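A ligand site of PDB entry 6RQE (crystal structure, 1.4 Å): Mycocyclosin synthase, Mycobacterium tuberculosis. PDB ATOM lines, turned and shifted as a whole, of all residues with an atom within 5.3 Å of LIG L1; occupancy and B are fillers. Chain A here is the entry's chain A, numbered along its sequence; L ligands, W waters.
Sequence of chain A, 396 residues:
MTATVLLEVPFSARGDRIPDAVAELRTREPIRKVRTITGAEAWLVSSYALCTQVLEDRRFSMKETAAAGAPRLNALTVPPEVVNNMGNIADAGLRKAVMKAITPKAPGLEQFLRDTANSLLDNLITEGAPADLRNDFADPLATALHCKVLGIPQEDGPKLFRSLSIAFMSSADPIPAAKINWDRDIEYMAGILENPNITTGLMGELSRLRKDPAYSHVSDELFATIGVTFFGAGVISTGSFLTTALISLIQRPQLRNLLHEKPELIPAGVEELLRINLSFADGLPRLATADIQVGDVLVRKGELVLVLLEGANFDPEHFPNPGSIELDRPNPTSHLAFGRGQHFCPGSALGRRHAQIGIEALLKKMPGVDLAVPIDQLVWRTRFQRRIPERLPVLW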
ATOM      1  N   MET A  62      24.379 -23.312  39.704  1.00  0.00           N
ATOM      2  CA  MET A  62      23.630 -23.405  38.460  1.00  0.00           C
ATOM      3  C   MET A  62      22.145 -23.143  38.730  1.00  0.00           C
ATOM      4  O   MET A  62      21.486 -22.354  38.030  1.00  0.00           O
ATOM      5  CB  MET A  62      23.823 -24.771  37.775  1.00  0.00           C
ATOM      6  CG  MET A  62      22.797 -25.053  36.625  1.00  0.00           C
ATOM      7  SD  MET A  62      22.924 -26.714  35.893  1.00  0.00           S
ATOM      8  CE  MET A  62      24.467 -26.479  35.083  1.00  0.00           C
ATOM      9  N   THR A  77      14.629 -21.274  28.168  1.00  0.00           N
ATOM     10  CA  THR A  77      13.836 -21.980  27.172  1.00  0.00           C
ATOM     11  C   THR A  77      13.155 -23.209  27.734  1.00  0.00           C
ATOM     12  O   THR A  77      12.480 -23.923  26.994  1.00  0.00           O
ATOM     13  CB  THR A  77      14.675 -22.390  25.976  1.00  0.00           C
ATOM     14  OG1 THR A  77      15.626 -23.372  26.363  1.00  0.00           O
ATOM     15  CG2 THR A  77      15.423 -21.182  25.360  1.00  0.00           C
ATOM     16  N   VAL A  78      13.272 -23.426  29.049  1.00  0.00           N
ATOM     17  CA  VAL A  78      12.655 -24.532  29.764  1.00  0.00           C
ATOM     18  C   VAL A  78      12.035 -23.962  31.030  1.00  0.00           C
ATOM     19  O   VAL A  78      12.392 -22.864  31.474  1.00  0.00           O
ATOM     20  CB  VAL A  78      13.700 -25.614  30.138  1.00  0.00           C
ATOM     21  CG1 VAL A  78      14.296 -26.223  28.882  1.00  0.00           C
ATOM     22  CG2 VAL A  78      14.820 -25.045  31.015  1.00  0.00           C
ATOM     23  N   VAL A  82      13.544 -26.946  35.694  1.00  0.00           N
ATOM     24  CA  VAL A  82      14.373 -27.812  34.857  1.00  0.00           C
ATOM     25  C   VAL A  82      15.822 -27.379  34.837  1.00  0.00           C
ATOM     26  O   VAL A  82      16.701 -28.152  34.482  1.00  0.00           O
ATOM     27  CB  VAL A  82      13.716 -27.907  33.458  1.00  0.00           C
ATOM     28  CG1 VAL A  82      14.540 -28.760  32.491  1.00  0.00           C
ATOM     29  CG2 VAL A  82      12.298 -28.455  33.544  1.00  0.00           C
ATOM     30  N   VAL A  83      16.133 -26.138  35.218  1.00  0.00           N
ATOM     31  CA  VAL A  83      17.540 -25.787  35.337  1.00  0.00           C
ATOM     32  C   VAL A  83      18.215 -26.640  36.407  1.00  0.00           C
ATOM     33  O   VAL A  83      19.415 -26.935  36.307  1.00  0.00           O
ATOM     34  CB  VAL A  83      17.681 -24.269  35.626  1.00  0.00           C
ATOM     35  CG1 VAL A  83      19.128 -23.897  35.873  1.00  0.00           C
ATOM     36  CG2 VAL A  83      17.131 -23.475  34.433  1.00  0.00           C
ATOM     37  N   ASN A  85      17.681 -29.813  36.786  1.00  0.00           N
ATOM     38  CA  ASN A  85      17.316 -31.147  36.317  1.00  0.00           C
ATOM     39  C   ASN A  85      18.096 -32.226  37.034  1.00  0.00           C
ATOM     40  O   ASN A  85      17.515 -33.204  37.537  1.00  0.00           O
ATOM     41  CB  ASN A  85      17.571 -31.198  34.807  1.00  0.00           C
ATOM     42  CG  ASN A  85      16.910 -32.367  34.103  1.00  0.00           C
ATOM     43  OD1 ASN A  85      15.809 -32.786  34.444  1.00  0.00           O
ATOM     44  ND2 ASN A  85      17.586 -32.879  33.102  1.00  0.00           N
ATOM     45  N   MET A  86      19.417 -32.102  37.104  1.00  0.00           N
ATOM     46  CA  MET A  86      20.183 -33.187  37.720  1.00  0.00           C
ATOM     47  C   MET A  86      19.932 -33.288  39.222  1.00  0.00           C
ATOM     48  O   MET A  86      19.915 -34.389  39.769  1.00  0.00           O
ATOM     49  CB  MET A  86      21.675 -33.077  37.404  1.00  0.00           C
ATOM     50  CG  MET A  86      22.055 -33.499  35.972  1.00  0.00           C
ATOM     51  SD  MET A  86      21.728 -35.221  35.506  1.00  0.00           S
ATOM     52  CE  MET A  86      22.430 -36.123  36.894  1.00  0.00           C
ATOM     53  N   ALA A 167      15.042 -24.775  20.804  1.00  0.00           N
ATOM     54  CA  ALA A 167      15.233 -25.084  22.221  1.00  0.00           C
ATOM     55  C   ALA A 167      16.554 -24.617  22.753  1.00  0.00           C
ATOM     56  O   ALA A 167      16.678 -24.244  23.926  1.00  0.00           O
ATOM     57  CB  ALA A 167      15.078 -26.595  22.423  1.00  0.00           C
ATOM     58  N   PHE A 168      17.589 -24.670  21.914  1.00  0.00           N
ATOM     59  CA  PHE A 168      18.917 -24.272  22.323  1.00  0.00           C
ATOM     60  C   PHE A 168      19.309 -22.911  21.797  1.00  0.00           C
ATOM     61  O   PHE A 168      20.479 -22.566  21.788  1.00  0.00           O
ATOM     62  CB  PHE A 168      19.923 -25.366  21.976  1.00  0.00           C
ATOM     63  CG  PHE A 168      19.797 -26.541  22.901  1.00  0.00           C
ATOM     64  CD1 PHE A 168      20.476 -26.537  24.104  1.00  0.00           C
ATOM     65  CD2 PHE A 168      18.911 -27.541  22.632  1.00  0.00           C
ATOM     66  CE1 PHE A 168      20.322 -27.597  25.000  1.00  0.00           C
ATOM     67  CE2 PHE A 168      18.744 -28.607  23.578  1.00  0.00           C
ATOM     68  CZ  PHE A 168      19.450 -28.594  24.727  1.00  0.00           C
ATOM     69  N   TRP A 182       8.309 -27.579  23.625  1.00  0.00           N
ATOM     70  CA  TRP A 182       8.529 -28.240  24.923  1.00  0.00           C
ATOM     71  C   TRP A 182       7.286 -28.995  25.358  1.00  0.00           C
ATOM     72  O   TRP A 182       7.357 -30.191  25.726  1.00  0.00           O
ATOM     73  CB  TRP A 182       8.928 -27.208  25.974  1.00  0.00           C
ATOM     74  CG  TRP A 182       9.098 -27.806  27.347  1.00  0.00           C
ATOM     75  CD1 TRP A 182       8.160 -27.847  28.338  1.00  0.00           C
ATOM     76  CD2 TRP A 182      10.254 -28.449  27.851  1.00  0.00           C
ATOM     77  NE1 TRP A 182       8.689 -28.486  29.435  1.00  0.00           N
ATOM     78  CE2 TRP A 182       9.973 -28.854  29.164  1.00  0.00           C
ATOM     79  CE3 TRP A 182      11.532 -28.712  27.331  1.00  0.00           C
ATOM     80  CZ2 TRP A 182      10.901 -29.526  29.952  1.00  0.00           C
ATOM     81  CZ3 TRP A 182      12.459 -29.371  28.130  1.00  0.00           C
ATOM     82  CH2 TRP A 182      12.124 -29.781  29.412  1.00  0.00           C
ATOM     83  N   VAL A 228      12.956 -35.745  27.595  1.00  0.00           N
ATOM     84  CA  VAL A 228      13.103 -34.589  26.694  1.00  0.00           C
ATOM     85  C   VAL A 228      14.492 -33.974  26.858  1.00  0.00           C
ATOM     86  O   VAL A 228      15.149 -33.634  25.861  1.00  0.00           O
ATOM     87  CB  VAL A 228      11.997 -33.542  26.947  1.00  0.00           C
ATOM     88  CG1 VAL A 228      12.242 -32.303  26.068  1.00  0.00           C
ATOM     89  CG2 VAL A 228      10.643 -34.112  26.687  1.00  0.00           C
ATOM     90  N   THR A 229      14.939 -33.796  28.096  1.00  0.00           N
ATOM     91  CA  THR A 229      16.197 -33.108  28.357  1.00  0.00           C
ATOM     92  C   THR A 229      17.396 -33.937  27.912  1.00  0.00           C
ATOM     93  O   THR A 229      18.368 -33.393  27.366  1.00  0.00           O
ATOM     94  CB  THR A 229      16.352 -32.690  29.827  1.00  0.00           C
ATOM     95  OG1 THR A 229      16.232 -33.837  30.674  1.00  0.00           O
ATOM     96  CG2 THR A 229      15.326 -31.650  30.208  1.00  0.00           C
ATOM     97  N   GLY A 232      17.526 -33.882  24.120  1.00  0.00           N
ATOM     98  CA  GLY A 232      17.892 -32.598  23.533  1.00  0.00           C
ATOM     99  C   GLY A 232      19.320 -32.231  23.839  1.00  0.00           C
ATOM    100  O   GLY A 232      20.099 -31.882  22.926  1.00  0.00           O
ATOM    101  N   ALA A 233      19.739 -32.329  25.099  1.00  0.00           N
ATOM    102  CA  ALA A 233      21.114 -31.991  25.455  1.00  0.00           C
ATOM    103  C   ALA A 233      22.090 -32.932  24.775  1.00  0.00           C
ATOM    104  O   ALA A 233      23.140 -32.514  24.265  1.00  0.00           O
ATOM    105  CB  ALA A 233      21.298 -32.019  26.970  1.00  0.00           C
ATOM    106  N   SER A 237      24.526 -31.638  21.765  1.00  0.00           N
ATOM    107  CA  SER A 237      25.909 -31.557  22.175  1.00  0.00           C
ATOM    108  C   SER A 237      26.785 -32.483  21.331  1.00  0.00           C
ATOM    109  O   SER A 237      27.862 -32.082  20.896  1.00  0.00           O
ATOM    110  CB  SER A 237      26.082 -31.902  23.652  1.00  0.00           C
ATOM    111  OG  SER A 237      25.363 -30.970  24.460  1.00  0.00           O
ATOM    112  N   PHE A 280      30.522 -24.801  22.567  1.00  0.00           N
ATOM    113  CA  PHE A 280      29.726 -23.992  23.482  1.00  0.00           C
ATOM    114  C   PHE A 280      29.880 -22.533  23.152  1.00  0.00           C
ATOM    115  O   PHE A 280      30.977 -21.983  23.203  1.00  0.00           O
ATOM    116  CB  PHE A 280      30.061 -24.270  24.950  1.00  0.00           C
ATOM    117  CG  PHE A 280      29.293 -25.432  25.518  1.00  0.00           C
ATOM    118  CD1 PHE A 280      29.520 -26.715  25.050  1.00  0.00           C
ATOM    119  CD2 PHE A 280      28.351 -25.244  26.516  1.00  0.00           C
ATOM    120  CE1 PHE A 280      28.795 -27.784  25.573  1.00  0.00           C
ATOM    121  CE2 PHE A 280      27.639 -26.309  27.036  1.00  0.00           C
ATOM    122  CZ  PHE A 280      27.856 -27.565  26.561  1.00  0.00           C
ATOM    123  N   GLN A 385      23.038 -21.623  21.572  1.00  0.00           N
ATOM    124  CA  GLN A 385      23.872 -22.083  22.686  1.00  0.00           C
ATOM    125  C   GLN A 385      25.054 -22.914  22.208  1.00  0.00           C
ATOM    126  O   GLN A 385      25.940 -23.217  23.014  1.00  0.00           O
ATOM    127  CB  GLN A 385      23.061 -22.858  23.690  1.00  0.00           C
ATOM    128  CG  GLN A 385      22.013 -22.000  24.455  1.00  0.00           C
ATOM    129  CD  GLN A 385      21.140 -22.805  25.376  1.00  0.00           C
ATOM    130  OE1 GLN A 385      21.599 -23.735  26.063  1.00  0.00           O
ATOM    131  NE2 GLN A 385      19.837 -22.493  25.381  1.00  0.00           N
ATOM    132  N   ARG A 386      25.070 -23.257  20.943  1.00  0.00           N
ATOM    133  CA  ARG A 386      26.222 -23.945  20.330  1.00  0.00           C
ATOM    134  C   ARG A 386      26.655 -23.161  19.103  1.00  0.00           C
ATOM    135  O   ARG A 386      25.872 -22.400  18.574  1.00  0.00           O
ATOM    136  CB  ARG A 386      25.828 -25.354  19.867  1.00  0.00           C
ATOM    137  CG  ARG A 386      25.468 -26.293  21.012  1.00  0.00           C
ATOM    138  CD  ARG A 386      26.614 -26.593  21.995  1.00  0.00           C
ATOM    139  NE  ARG A 386      26.198 -27.547  23.014  1.00  0.00           N
ATOM    140  CZ  ARG A 386      25.517 -27.206  24.083  1.00  0.00           C
ATOM    141  NH1 ARG A 386      25.245 -25.932  24.292  1.00  0.00           N
ATOM    142  NH2 ARG A 386      25.120 -28.117  24.926  1.00  0.00           N
HETATM  143  C1  LIG L   1      22.838 -26.954  28.270  1.00  0.00           C
HETATM  144  C2  LIG L   1      22.107 -25.937  28.896  1.00  0.00           C
HETATM  145  C3  LIG L   1      21.798 -26.017  30.201  1.00  0.00           C
HETATM  146  C4  LIG L   1      22.179 -27.119  30.972  1.00  0.00           C
HETATM  147  C5  LIG L   1      21.800 -27.079  32.444  1.00  0.00           C
HETATM  148  C6  LIG L   1      20.452 -27.640  32.745  1.00  0.00           C
HETATM  149  C7  LIG L   1      19.287 -27.006  32.072  1.00  0.00           C
HETATM  150  C8  LIG L   1      18.949 -29.109  30.849  1.00  0.00           C
HETATM  151  C9  LIG L   1      19.442 -29.174  29.375  1.00  0.00           C
HETATM  152  C10 LIG L   1      18.445 -28.694  28.374  1.00  0.00           C
HETATM  153  C11 LIG L   1      17.716 -29.733  27.826  1.00  0.00           C
HETATM  154  C12 LIG L   1      16.710 -29.518  26.869  1.00  0.00           C
HETATM  155  C13 LIG L   1      16.411 -28.225  26.528  1.00  0.00           C
HETATM  156  C14 LIG L   1      17.115 -27.185  27.073  1.00  0.00           C
HETATM  157  C15 LIG L   1      18.140 -27.422  27.995  1.00  0.00           C
HETATM  158  C16 LIG L   1      19.679 -29.840  31.939  1.00  0.00           C
HETATM  159  C17 LIG L   1      22.906 -28.087  30.331  1.00  0.00           C
HETATM  160  C18 LIG L   1      23.239 -28.003  29.005  1.00  0.00           C
HETATM  161  C19 LIG L   1      23.939 -28.978  28.373  1.00  0.00           C
HETATM  162  C20 LIG L   1      24.543 -29.802  27.843  1.00  0.00           C
HETATM  163  N1  LIG L   1      18.615 -27.745  31.218  1.00  0.00           N
HETATM  164  N2  LIG L   1      20.404 -29.091  32.801  1.00  0.00           N
HETATM  165  O1  LIG L   1      23.181 -26.877  26.996  1.00  0.00           O
HETATM  166  O2  LIG L   1      15.452 -27.992  25.668  1.00  0.00           O
HETATM  167  O3  LIG L   1      19.713 -30.932  32.005  1.00  0.00           O
HETATM  168  O4  LIG L   1      18.964 -25.890  32.242  1.00  0.00           O
HETATM  169  C1  LG2 L   2      26.143 -31.062  30.986  1.00  0.00           C
HETATM  170  C2  LG2 L   2      29.239 -30.883  27.273  1.00  0.00           C
HETATM  171  C3  LG2 L   2      27.261 -34.967  25.530  1.00  0.00           C
HETATM  172  C4  LG2 L   2      23.742 -34.591  28.767  1.00  0.00           C
HETATM  173  C5  LG2 L   2      27.228 -30.697  30.183  1.00  0.00           C
HETATM  174  C6  LG2 L   2      28.158 -29.650  30.444  1.00  0.00           C
HETATM  175  C7  LG2 L   2      29.008 -29.598  29.401  1.00  0.00           C
HETATM  176  C8  LG2 L   2      28.622 -30.598  28.474  1.00  0.00           C
HETATM  177  C9  LG2 L   2      30.137 -28.611  29.268  1.00  0.00           C
HETATM  178  C10 LG2 L   2      28.198 -28.786  31.713  1.00  0.00           C
HETATM  179  C11 LG2 L   2      27.221 -27.609  31.658  1.00  0.00           C
HETATM  180  C12 LG2 L   2      27.378 -26.764  32.892  1.00  0.00           C
HETATM  181  O1  LG2 L   2      28.095 -27.123  33.819  1.00  0.00           O
HETATM  182  O2  LG2 L   2      26.826 -25.691  32.996  1.00  0.00           O
HETATM  183  C13 LG2 L   2      28.995 -31.991  26.409  1.00  0.00           C
HETATM  184  C14 LG2 L   2      29.680 -32.321  25.237  1.00  0.00           C
HETATM  185  C15 LG2 L   2      29.125 -33.447  24.746  1.00  0.00           C
HETATM  186  C16 LG2 L   2      28.071 -33.824  25.637  1.00  0.00           C
HETATM  187  C17 LG2 L   2      30.825 -31.530  24.640  1.00  0.00           C
HETATM  188  C18 LG2 L   2      29.428 -34.224  23.551  1.00  0.00           C
HETATM  189  C19 LG2 L   2      30.631 -34.306  23.136  1.00  0.00           C
HETATM  190  C20 LG2 L   2      26.132 -35.296  26.272  1.00  0.00           C
HETATM  191  C21 LG2 L   2      25.325 -36.443  26.143  1.00  0.00           C
HETATM  192  C22 LG2 L   2      24.306 -36.312  27.062  1.00  0.00           C
HETATM  193  C23 LG2 L   2      24.537 -35.114  27.767  1.00  0.00           C
HETATM  194  C24 LG2 L   2      25.597 -37.528  25.130  1.00  0.00           C
HETATM  195  C25 LG2 L   2      23.175 -37.191  27.389  1.00  0.00           C
HETATM  196  C26 LG2 L   2      22.751 -38.122  26.637  1.00  0.00           C
HETATM  197  C27 LG2 L   2      24.087 -33.546  29.622  1.00  0.00           C
HETATM  198  C28 LG2 L   2      23.230 -33.133  30.714  1.00  0.00           C
HETATM  199  C29 LG2 L   2      23.879 -32.154  31.320  1.00  0.00           C
HETATM  200  C30 LG2 L   2      25.148 -31.964  30.605  1.00  0.00           C
HETATM  201  C31 LG2 L   2      21.861 -33.702  31.015  1.00  0.00           C
HETATM  202  C32 LG2 L   2      23.420 -31.353  32.481  1.00  0.00           C
HETATM  203  C33 LG2 L   2      24.125 -31.835  33.705  1.00  0.00           C
HETATM  204  C34 LG2 L   2      23.651 -30.946  34.798  1.00  0.00           C
HETATM  205  O3  LG2 L   2      24.111 -31.115  35.873  1.00  0.00           O
HETATM  206  O4  LG2 L   2      22.807 -30.063  34.720  1.00  0.00           O
HETATM  207  N1  LG2 L   2      27.533 -31.273  28.964  1.00  0.00           N
HETATM  208  N2  LG2 L   2      28.152 -32.956  26.617  1.00  0.00           N
HETATM  209  N3  LG2 L   2      25.657 -34.526  27.273  1.00  0.00           N
HETATM  210  N4  LG2 L   2      25.233 -32.883  29.665  1.00  0.00           N
HETATM  211 FE1  LG2 L   2      26.721 -33.016  28.270  1.00  0.00          FE
HETATM  212  O   HOH W   1      14.212 -29.699  24.127  1.00  0.00           O
HETATM  213  O   HOH W   2      18.544 -23.857  30.497  1.00  0.00           O
HETATM  214  O   HOH W   3      13.427 -25.862  25.204  1.00  0.00           O
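N2 of LIG L1 sits at hydrogen-bond distance from O4 of LG2 L2 (3.2 Å).
The side-chain hydroxyl (OG1) of Thr 229 lies within hydrogen-bond range of the side-chain amide nitrogen (ND2) of Asn 85 (2.9 Å).
The side-chain hydroxyl of Ser 237 lies within hydrogen-bond range of the guanidinium group of Arg 386 (2.9 Å).
The backbone carbonyl oxygen (O) of Phe 168 is in hydrogen-bond range of the backbone NH (N) of Gln 385 (2.7 Å).
O of Ala 167 sits at hydrogen-bond distance from OG1 of Thr 77, at 2.8 Å.
The side-chain hydroxyl of Ser 237 sits at hydrogen-bond distance from the backbone carbonyl oxygen of Ala 233 (2.7 Å).
The side-chain amide nitrogen of Asn 85 sits at hydrogen-bond distance from an oxygen (O3) of LIG L1 (3.1 Å).
The guanidinium group of Arg 386 lies within hydrogen-bond range of an oxygen (O1) of LIG L1, at 3.1 Å.
Met 62 touches LIG L1.
CG1 of Val 78 touches C14 of LIG L1 (3.5 Å).
Val 82 touches LIG L1 (O to C7, 3.7 Å).
Val 83 touches LIG L1.
Ala 167 touches LIG L1.
CZ of Phe 168 touches C13 of LIG L1, 3.6 Å away.
CA of Thr 229 touches C11 of LIG L1, 3.7 Å away.
Ser 237 touches LIG L1 (OG to C20, 3.7 Å).
Gln 385 touches LIG L1.
Hydrophobic or aromatic side chains that line LIG L1: Met 62, Val 78, Val 83, Ala 167 and Phe 168.
11 residues have an atom within 4 Å of LIG L1: Met 62, Val 78, Val 82, Val 83, Asn 85, Ala 167, Phe 168, Thr 229, Ser 237, Gln 385 and Arg 386.
Water W3 lies within hydrogen-bond range of O of Thr 77 (2.8 Å) and O2 of LIG L1 (3.0 Å).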
